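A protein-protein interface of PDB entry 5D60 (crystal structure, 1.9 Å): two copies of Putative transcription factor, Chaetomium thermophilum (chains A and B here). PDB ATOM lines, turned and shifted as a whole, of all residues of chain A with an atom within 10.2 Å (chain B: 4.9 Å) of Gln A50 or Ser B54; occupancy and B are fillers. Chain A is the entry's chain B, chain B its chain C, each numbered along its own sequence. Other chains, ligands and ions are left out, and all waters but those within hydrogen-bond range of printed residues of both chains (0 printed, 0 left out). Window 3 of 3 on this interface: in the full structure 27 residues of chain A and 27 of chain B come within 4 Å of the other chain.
Printed residues of chain B within 4 Å of Ala A49: Asn B51. Gln A50 touches just these residues of chain B: Gln B50 (3.3 Å), Asn B51 (2.9 Å) and Ser B54 (3.0 Å). Gln A52 touches none of the printed residues of chain B. Ser A54 touches none of the printed residues of chain B. Of the printed residues of chain A, Val B47 touches Met A46 (3.6 Å) and Val A47 (3.8 Å). Of chain A, only Met A46 (3.2 Å), Ala A49 (3.96 Å) and Gln A50 (2.9 Å) come within 4 Å of Asn B51. No residue of chain A comes within 4 Å of Ala B53. No residue of chain A comes within 4 Å of Asn B55. No residue of chain A comes within 4 Å of Ile B57. The nearest residue of chain B that does not touch Gln A50 is Val B47 (4.4 Å).
Among the printed residues, merely in contact across the chains: Met A46 with Val B47 (3.6 Å), Val A47 with Val B47 (3.8 Å), Ala A49 with Asn B51 (3.96 Å), Ala A53 with Ser B54 (3.7 Å), Ala A53 with Ile B58 (3.7 Å), Glu A56 with Ile B58 (3.4 Å), Ile A57 with Ser B54 (3.9 Å) and Ile A57 with Ile B58 (3.9 Å).
The backbone carbonyl oxygen (O) of Met A46 lies within hydrogen-bond range of the side-chain amide nitrogen (ND2) of Asn B51 (3.2 Å). NE2 of Gln A50 is in hydrogen-bond range of O of Gln B50. The side-chain amide oxygen (OD1) of Asn B51 sits close to the backbone NH (N) of Gln A50 (3.3 Å). The side-chain amide nitrogen (NE2) of Gln A50 lies within hydrogen-bond range of the side-chain hydroxyl (OG) of Ser B54.
Of the 10 printed residues of chain B, 5 touch a printed residue of chain A. Hydrophobic or aromatic side chains of chain B within 4 Å of the printed part of chain A: Val B47 and Ile B58. Among the printed residues, no Asp or Glu carboxylate lies within 4 Å of a Lys or Arg side-chain nitrogen of the other chain.
Val A47 touches its own counterpart, Val B47. Gln A50 touches Asn B51, but with the chains exchanged Asn A51 does not touch Gln B50 (8.4 Å). Gln A50 touches Ser B54, but with the chains exchanged Ser A54 does not touch Gln B50 (7.8 Å). Ile A57 touches Ile B58, but with the chains exchanged Ile A58 does not touch Ile B57 (7.8 Å). Positions printed for both chains: 47, 50, 51, 52, 53, 54, 55, 56, 57 and 58. Of the 12 pairs that touch across the chains among the printed residues, 2 have their exchanged pair printed and touching as well.
The side-chain amide oxygen of Gln A50 is in hydrogen-bond range of the side-chain hydroxyl of Ser A54. O of Gln B50 lies close to OG of Ser B54, at 3.4 Å.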
ATOM      1  N   THR A  42      10.944 -30.686 -12.851  1.00  0.00           N
ATOM      2  CA  THR A  42      11.842 -30.058 -11.917  1.00  0.00           C
ATOM      3  C   THR A  42      11.557 -28.570 -11.793  1.00  0.00           C
ATOM      4  O   THR A  42      11.566 -28.028 -10.711  1.00  0.00           O
ATOM      5  CB  THR A  42      13.310 -30.228 -12.366  1.00  0.00           C
ATOM      6  OG1 THR A  42      13.656 -31.604 -12.259  1.00  0.00           O
ATOM      7  CG2 THR A  42      14.247 -29.430 -11.471  1.00  0.00           C
ATOM      8  N   LEU A  43      11.244 -27.932 -12.916  1.00  0.00           N
ATOM      9  CA  LEU A  43      10.903 -26.547 -12.861  1.00  0.00           C
ATOM     10  C   LEU A  43       9.600 -26.316 -12.035  1.00  0.00           C
ATOM     11  O   LEU A  43       9.512 -25.396 -11.261  1.00  0.00           O
ATOM     12  CB  LEU A  43      10.753 -26.022 -14.287  1.00  0.00           C
ATOM     13  CG  LEU A  43      10.421 -24.514 -14.349  1.00  0.00           C
ATOM     14  CD1 LEU A  43      11.485 -23.690 -13.651  1.00  0.00           C
ATOM     15  CD2 LEU A  43      10.271 -24.173 -15.801  1.00  0.00           C
ATOM     16  N   GLN A  44       8.657 -27.235 -12.154  1.00  0.00           N
ATOM     17  CA  GLN A  44       7.433 -27.146 -11.405  1.00  0.00           C
ATOM     18  C   GLN A  44       7.648 -27.193  -9.885  1.00  0.00           C
ATOM     19  O   GLN A  44       7.134 -26.368  -9.110  1.00  0.00           O
ATOM     20  CB  GLN A  44       6.514 -28.254 -11.787  1.00  0.00           C
ATOM     21  CG  GLN A  44       5.819 -27.993 -13.103  1.00  0.00           C
ATOM     22  CD  GLN A  44       4.590 -28.866 -13.275  1.00  0.00           C
ATOM     23  OE1 GLN A  44       4.145 -29.599 -12.354  1.00  0.00           O
ATOM     24  NE2 GLN A  44       4.021 -28.788 -14.468  1.00  0.00           N
ATOM     25  N   LYS A  45       8.500 -28.135  -9.484  1.00  0.00           N
ATOM     26  CA  LYS A  45       9.019 -28.148  -8.098  1.00  0.00           C
ATOM     27  C   LYS A  45       9.611 -26.867  -7.593  1.00  0.00           C
ATOM     28  O   LYS A  45       9.329 -26.393  -6.481  1.00  0.00           O
ATOM     29  CB  LYS A  45      10.048 -29.291  -7.990  1.00  0.00           C
ATOM     30  CG  LYS A  45      10.678 -29.453  -6.603  1.00  0.00           C
ATOM     31  CD  LYS A  45      12.022 -30.178  -6.589  1.00  0.00           C
ATOM     32  CE  LYS A  45      13.191 -29.263  -7.010  1.00  0.00           C
ATOM     33  NZ  LYS A  45      13.416 -28.051  -6.152  1.00  0.00           N
ATOM     34  N   MET A  46      10.482 -26.280  -8.396  1.00  0.00           N
ATOM     35  CA  MET A  46      11.092 -25.059  -8.025  1.00  0.00           C
ATOM     36  C   MET A  46      10.121 -23.911  -7.902  1.00  0.00           C
ATOM     37  O   MET A  46      10.256 -23.061  -7.030  1.00  0.00           O
ATOM     38  CB  MET A  46      12.183 -24.739  -9.041  1.00  0.00           C
ATOM     39  CG  MET A  46      13.303 -25.739  -9.012  1.00  0.00           C
ATOM     40  SD  MET A  46      14.507 -25.513 -10.337  1.00  0.00           S
ATOM     41  CE  MET A  46      16.024 -26.124  -9.588  1.00  0.00           C
ATOM     42  N   VAL A  47       9.170 -23.830  -8.834  1.00  0.00           N
ATOM     43  CA  VAL A  47       8.198 -22.735  -8.851  1.00  0.00           C
ATOM     44  C   VAL A  47       7.215 -22.873  -7.671  1.00  0.00           C
ATOM     45  O   VAL A  47       6.953 -21.920  -6.995  1.00  0.00           O
ATOM     46  CB  VAL A  47       7.461 -22.682 -10.191  1.00  0.00           C
ATOM     47  CG1 VAL A  47       6.307 -21.720 -10.131  1.00  0.00           C
ATOM     48  CG2 VAL A  47       8.435 -22.184 -11.303  1.00  0.00           C
ATOM     49  N   LYS A  48       6.759 -24.093  -7.395  1.00  0.00           N
ATOM     50  CA  LYS A  48       6.119 -24.380  -6.104  1.00  0.00           C
ATOM     51  C   LYS A  48       6.886 -23.892  -4.874  1.00  0.00           C
ATOM     52  O   LYS A  48       6.314 -23.258  -3.981  1.00  0.00           O
ATOM     53  CB  LYS A  48       5.926 -25.894  -5.992  1.00  0.00           C
ATOM     54  CG  LYS A  48       4.594 -26.380  -6.458  1.00  0.00           C
ATOM     55  CD  LYS A  48       4.680 -27.736  -7.110  1.00  0.00           C
ATOM     56  CE  LYS A  48       3.292 -28.152  -7.571  1.00  0.00           C
ATOM     57  NZ  LYS A  48       3.227 -29.399  -8.390  1.00  0.00           N
ATOM     58  N   ALA A  49       8.157 -24.267  -4.768  1.00  0.00           N
ATOM     59  CA  ALA A  49       8.986 -23.836  -3.673  1.00  0.00           C
ATOM     60  C   ALA A  49       8.971 -22.314  -3.565  1.00  0.00           C
ATOM     61  O   ALA A  49       8.874 -21.748  -2.480  1.00  0.00           O
ATOM     62  CB  ALA A  49      10.400 -24.370  -3.826  1.00  0.00           C
ATOM     63  N   GLN A  50       8.962 -21.634  -4.707  1.00  0.00           N
ATOM     64  CA  GLN A  50       8.841 -20.190  -4.721  1.00  0.00           C
ATOM     65  C   GLN A  50       7.526 -19.717  -4.143  1.00  0.00           C
ATOM     66  O   GLN A  50       7.465 -18.727  -3.451  1.00  0.00           O
ATOM     67  CB  GLN A  50       8.868 -19.716  -6.172  1.00  0.00           C
ATOM     68  CG  GLN A  50       9.678 -18.508  -6.497  1.00  0.00           C
ATOM     69  CD  GLN A  50       9.530 -17.399  -5.499  1.00  0.00           C
ATOM     70  OE1 GLN A  50       8.432 -16.903  -5.209  1.00  0.00           O
ATOM     71  NE2 GLN A  50      10.652 -16.984  -4.968  1.00  0.00           N
ATOM     72  N   ASN A  51       6.463 -20.362  -4.531  1.00  0.00           N
ATOM     73  CA  ASN A  51       5.183 -20.038  -4.001  1.00  0.00           C
ATOM     74  C   ASN A  51       5.155 -20.156  -2.460  1.00  0.00           C
ATOM     75  O   ASN A  51       4.620 -19.294  -1.777  1.00  0.00           O
ATOM     76  CB  ASN A  51       4.143 -20.964  -4.553  1.00  0.00           C
ATOM     77  CG  ASN A  51       2.756 -20.396  -4.419  1.00  0.00           C
ATOM     78  OD1 ASN A  51       2.540 -19.403  -3.714  1.00  0.00           O
ATOM     79  ND2 ASN A  51       1.795 -21.025  -5.084  1.00  0.00           N
ATOM     80  N   GLN A  52       5.775 -21.199  -1.918  1.00  0.00           N
ATOM     81  CA  GLN A  52       5.900 -21.361  -0.454  1.00  0.00           C
ATOM     82  C   GLN A  52       6.728 -20.281   0.185  1.00  0.00           C
ATOM     83  O   GLN A  52       6.392 -19.783   1.261  1.00  0.00           O
ATOM     84  CB  GLN A  52       6.541 -22.701  -0.134  1.00  0.00           C
ATOM     85  CG  GLN A  52       5.634 -23.858  -0.470  1.00  0.00           C
ATOM     86  CD  GLN A  52       6.236 -25.183  -0.024  1.00  0.00           C
ATOM     87  OE1 GLN A  52       7.459 -25.327   0.023  1.00  0.00           O
ATOM     88  NE2 GLN A  52       5.386 -26.149   0.316  1.00  0.00           N
ATOM     89  N   ALA A  53       7.830 -19.914  -0.459  1.00  0.00           N
ATOM     90  CA  ALA A  53       8.638 -18.851   0.035  1.00  0.00           C
ATOM     91  C   ALA A  53       7.856 -17.553   0.046  1.00  0.00           C
ATOM     92  O   ALA A  53       7.998 -16.747   0.970  1.00  0.00           O
ATOM     93  CB  ALA A  53       9.900 -18.702  -0.805  1.00  0.00           C
ATOM     94  N   SER A  54       7.070 -17.325  -1.001  1.00  0.00           N
ATOM     95  CA  SER A  54       6.224 -16.143  -1.108  1.00  0.00           C
ATOM     96  C   SER A  54       5.276 -16.072   0.056  1.00  0.00           C
ATOM     97  O   SER A  54       5.220 -15.074   0.751  1.00  0.00           O
ATOM     98  CB  SER A  54       5.426 -16.158  -2.419  1.00  0.00           C
ATOM     99  OG  SER A  54       6.121 -15.467  -3.434  1.00  0.00           O
ATOM    100  N   ASN A  55       4.555 -17.162   0.279  1.00  0.00           N
ATOM    101  CA  ASN A  55       3.556 -17.210   1.343  1.00  0.00           C
ATOM    102  C   ASN A  55       4.170 -16.909   2.700  1.00  0.00           C
ATOM    103  O   ASN A  55       3.585 -16.187   3.503  1.00  0.00           O
ATOM    104  CB  ASN A  55       2.814 -18.550   1.340  1.00  0.00           C
ATOM    105  CG  ASN A  55       1.924 -18.722   0.098  1.00  0.00           C
ATOM    106  OD1 ASN A  55       1.544 -17.739  -0.567  1.00  0.00           O
ATOM    107  ND2 ASN A  55       1.570 -19.980  -0.208  1.00  0.00           N
ATOM    108  N   GLU A  56       5.329 -17.491   2.965  1.00  0.00           N
ATOM    109  CA  GLU A  56       6.004 -17.276   4.220  1.00  0.00           C
ATOM    110  C   GLU A  56       6.296 -15.818   4.412  1.00  0.00           C
ATOM    111  O   GLU A  56       6.160 -15.302   5.509  1.00  0.00           O
ATOM    112  CB  GLU A  56       7.323 -18.037   4.277  1.00  0.00           C
ATOM    113  CG  GLU A  56       7.163 -19.519   4.517  1.00  0.00           C
ATOM    114  CD  GLU A  56       8.496 -20.235   4.717  1.00  0.00           C
ATOM    115  OE1 GLU A  56       9.516 -19.565   4.994  1.00  0.00           O
ATOM    116  OE2 GLU A  56       8.513 -21.486   4.609  1.00  0.00           O
ATOM    117  N   ILE A  57       6.735 -15.147   3.355  1.00  0.00           N
ATOM    118  CA  ILE A  57       6.919 -13.712   3.416  1.00  0.00           C
ATOM    119  C   ILE A  57       5.613 -13.045   3.818  1.00  0.00           C
ATOM    120  O   ILE A  57       5.567 -12.297   4.800  1.00  0.00           O
ATOM    121  CB  ILE A  57       7.403 -13.128   2.076  1.00  0.00           C
ATOM    122  CG1 ILE A  57       8.852 -13.582   1.805  1.00  0.00           C
ATOM    123  CG2 ILE A  57       7.318 -11.608   2.116  1.00  0.00           C
ATOM    124  CD1 ILE A  57       9.240 -13.512   0.344  1.00  0.00           C
ATOM    125  N   ILE A  58       4.554 -13.348   3.085  1.00  0.00           N
ATOM    126  CA  ILE A  58       3.235 -12.804   3.390  1.00  0.00           C
ATOM    127  C   ILE A  58       2.882 -12.995   4.862  1.00  0.00           C
ATOM    128  O   ILE A  58       2.393 -12.070   5.499  1.00  0.00           O
ATOM    129  CB  ILE A  58       2.146 -13.398   2.480  1.00  0.00           C
ATOM    130  CG1 ILE A  58       2.350 -12.943   1.028  1.00  0.00           C
ATOM    131  CG2 ILE A  58       0.751 -12.985   2.953  1.00  0.00           C
ATOM    132  CD1 ILE A  58       1.556 -13.747   0.013  1.00  0.00           C
ATOM    133  N   HIS A  60       4.813 -13.274   7.457  1.00  0.00           N
ATOM    134  CA  HIS A  60       5.708 -12.505   8.320  1.00  0.00           C
ATOM    135  C   HIS A  60       5.520 -10.991   8.089  1.00  0.00           C
ATOM    136  O   HIS A  60       6.137 -10.194   8.784  1.00  0.00           O
ATOM    137  CB  HIS A  60       7.164 -12.932   8.103  1.00  0.00           C
ATOM    138  N   VAL B  47      14.488 -19.210 -11.575  1.00  0.00           N
ATOM    139  CA  VAL B  47      13.547 -19.457 -10.442  1.00  0.00           C
ATOM    140  C   VAL B  47      14.364 -19.742  -9.185  1.00  0.00           C
ATOM    141  O   VAL B  47      14.028 -19.282  -8.107  1.00  0.00           O
ATOM    142  CB  VAL B  47      12.543 -20.544 -10.780  1.00  0.00           C
ATOM    143  CG1 VAL B  47      11.756 -20.989  -9.541  1.00  0.00           C
ATOM    144  CG2 VAL B  47      11.551 -20.027 -11.824  1.00  0.00           C
ATOM    145  N   GLN B  50      15.429 -16.500  -7.792  1.00  0.00           N
ATOM    146  CA  GLN B  50      14.291 -15.883  -7.135  1.00  0.00           C
ATOM    147  C   GLN B  50      14.044 -16.552  -5.758  1.00  0.00           C
ATOM    148  O   GLN B  50      13.792 -15.867  -4.765  1.00  0.00           O
ATOM    149  CB  GLN B  50      13.078 -16.084  -8.053  1.00  0.00           C
ATOM    150  CG  GLN B  50      12.964 -15.053  -9.213  1.00  0.00           C
ATOM    151  CD  GLN B  50      12.061 -15.523 -10.375  1.00  0.00           C
ATOM    152  OE1 GLN B  50      11.239 -16.422 -10.235  1.00  0.00           O
ATOM    153  NE2 GLN B  50      12.279 -14.950 -11.562  1.00  0.00           N
ATOM    154  N   ASN B  51      14.127 -17.867  -5.693  1.00  0.00           N
ATOM    155  CA  ASN B  51      13.968 -18.553  -4.381  1.00  0.00           C
ATOM    156  C   ASN B  51      15.033 -18.062  -3.385  1.00  0.00           C
ATOM    157  O   ASN B  51      14.741 -17.845  -2.213  1.00  0.00           O
ATOM    158  CB  ASN B  51      14.061 -20.079  -4.574  1.00  0.00           C
ATOM    159  CG  ASN B  51      12.861 -20.671  -5.294  1.00  0.00           C
ATOM    160  OD1 ASN B  51      11.775 -20.105  -5.280  1.00  0.00           O
ATOM    161  ND2 ASN B  51      13.049 -21.861  -5.896  1.00  0.00           N
ATOM    162  N   GLN B  52      16.268 -17.893  -3.832  1.00  0.00           N
ATOM    163  CA  GLN B  52      17.359 -17.424  -2.949  1.00  0.00           C
ATOM    164  C   GLN B  52      17.105 -16.028  -2.440  1.00  0.00           C
ATOM    165  O   GLN B  52      17.365 -15.720  -1.287  1.00  0.00           O
ATOM    166  CB  GLN B  52      18.685 -17.434  -3.700  1.00  0.00           C
ATOM    167  CG  GLN B  52      19.168 -18.842  -3.996  1.00  0.00           C
ATOM    168  CD  GLN B  52      20.419 -18.880  -4.824  1.00  0.00           C
ATOM    169  OE1 GLN B  52      20.950 -19.967  -5.180  1.00  0.00           O
ATOM    170  NE2 GLN B  52      20.884 -17.694  -5.202  1.00  0.00           N
ATOM    171  N   ALA B  53      16.623 -15.152  -3.315  1.00  0.00           N
ATOM    172  CA  ALA B  53      16.326 -13.819  -2.921  1.00  0.00           C
ATOM    173  C   ALA B  53      15.204 -13.821  -1.927  1.00  0.00           C
ATOM    174  O   ALA B  53      15.219 -13.034  -0.968  1.00  0.00           O
ATOM    175  CB  ALA B  53      15.938 -12.982  -4.140  1.00  0.00           C
ATOM    176  N   SER B  54      14.214 -14.660  -2.193  1.00  0.00           N
ATOM    177  CA  SER B  54      13.107 -14.828  -1.260  1.00  0.00           C
ATOM    178  C   SER B  54      13.642 -15.238   0.119  1.00  0.00           C
ATOM    179  O   SER B  54      13.295 -14.633   1.114  1.00  0.00           O
ATOM    180  CB  SER B  54      12.112 -15.869  -1.794  1.00  0.00           C
ATOM    181  OG  SER B  54      11.146 -15.211  -2.658  1.00  0.00           O
ATOM    182  N   ASN B  55      14.423 -16.308   0.159  1.00  0.00           N
ATOM    183  CA  ASN B  55      14.932 -16.846   1.432  1.00  0.00           C
ATOM    184  C   ASN B  55      15.677 -15.814   2.220  1.00  0.00           C
ATOM    185  O   ASN B  55      15.488 -15.719   3.448  1.00  0.00           O
ATOM    186  CB  ASN B  55      15.813 -18.084   1.237  1.00  0.00           C
ATOM    187  CG  ASN B  55      15.026 -19.301   0.764  1.00  0.00           C
ATOM    188  OD1 ASN B  55      13.790 -19.382   0.919  1.00  0.00           O
ATOM    189  ND2 ASN B  55      15.741 -20.261   0.166  1.00  0.00           N
ATOM    190  N   GLU B  56      16.489 -15.012   1.540  1.00  0.00           N
ATOM    191  CA  GLU B  56      17.234 -13.980   2.204  1.00  0.00           C
ATOM    192  C   GLU B  56      16.322 -12.998   2.884  1.00  0.00           C
ATOM    193  O   GLU B  56      16.581 -12.575   3.991  1.00  0.00           O
ATOM    194  CB  GLU B  56      18.112 -13.220   1.215  1.00  0.00           C
ATOM    195  CG  GLU B  56      19.347 -13.984   0.812  1.00  0.00           C
ATOM    196  CD  GLU B  56      20.309 -13.166  -0.019  1.00  0.00           C
ATOM    197  OE1 GLU B  56      20.139 -11.917  -0.122  1.00  0.00           O
ATOM    198  OE2 GLU B  56      21.256 -13.778  -0.569  1.00  0.00           O
ATOM    199  N   ILE B  57      15.236 -12.647   2.222  1.00  0.00           N
ATOM    200  CA  ILE B  57      14.232 -11.827   2.856  1.00  0.00           C
ATOM    201  C   ILE B  57      13.728 -12.521   4.120  1.00  0.00           C
ATOM    202  O   ILE B  57      13.772 -11.962   5.203  1.00  0.00           O
ATOM    203  CB  ILE B  57      13.077 -11.528   1.897  1.00  0.00           C
ATOM    204  CG1 ILE B  57      13.552 -10.596   0.782  1.00  0.00           C
ATOM    205  CG2 ILE B  57      11.933 -10.898   2.660  1.00  0.00           C
ATOM    206  CD1 ILE B  57      12.693 -10.652  -0.466  1.00  0.00           C
ATOM    207  N   ILE B  58      13.275 -13.757   3.972  1.00  0.00           N
ATOM    208  CA  ILE B  58      12.770 -14.547   5.102  1.00  0.00           C
ATOM    209  C   ILE B  58      13.782 -14.634   6.259  1.00  0.00           C
ATOM    210  O   ILE B  58      13.426 -14.411   7.395  1.00  0.00           O
ATOM    211  CB  ILE B  58      12.407 -15.987   4.676  1.00  0.00           C
ATOM    212  CG1 ILE B  58      11.210 -15.993   3.709  1.00  0.00           C
ATOM    213  CG2 ILE B  58      12.098 -16.861   5.900  1.00  0.00           C
ATOM    214  CD1 ILE B  58      11.023 -17.307   2.987  1.00  0.00           C
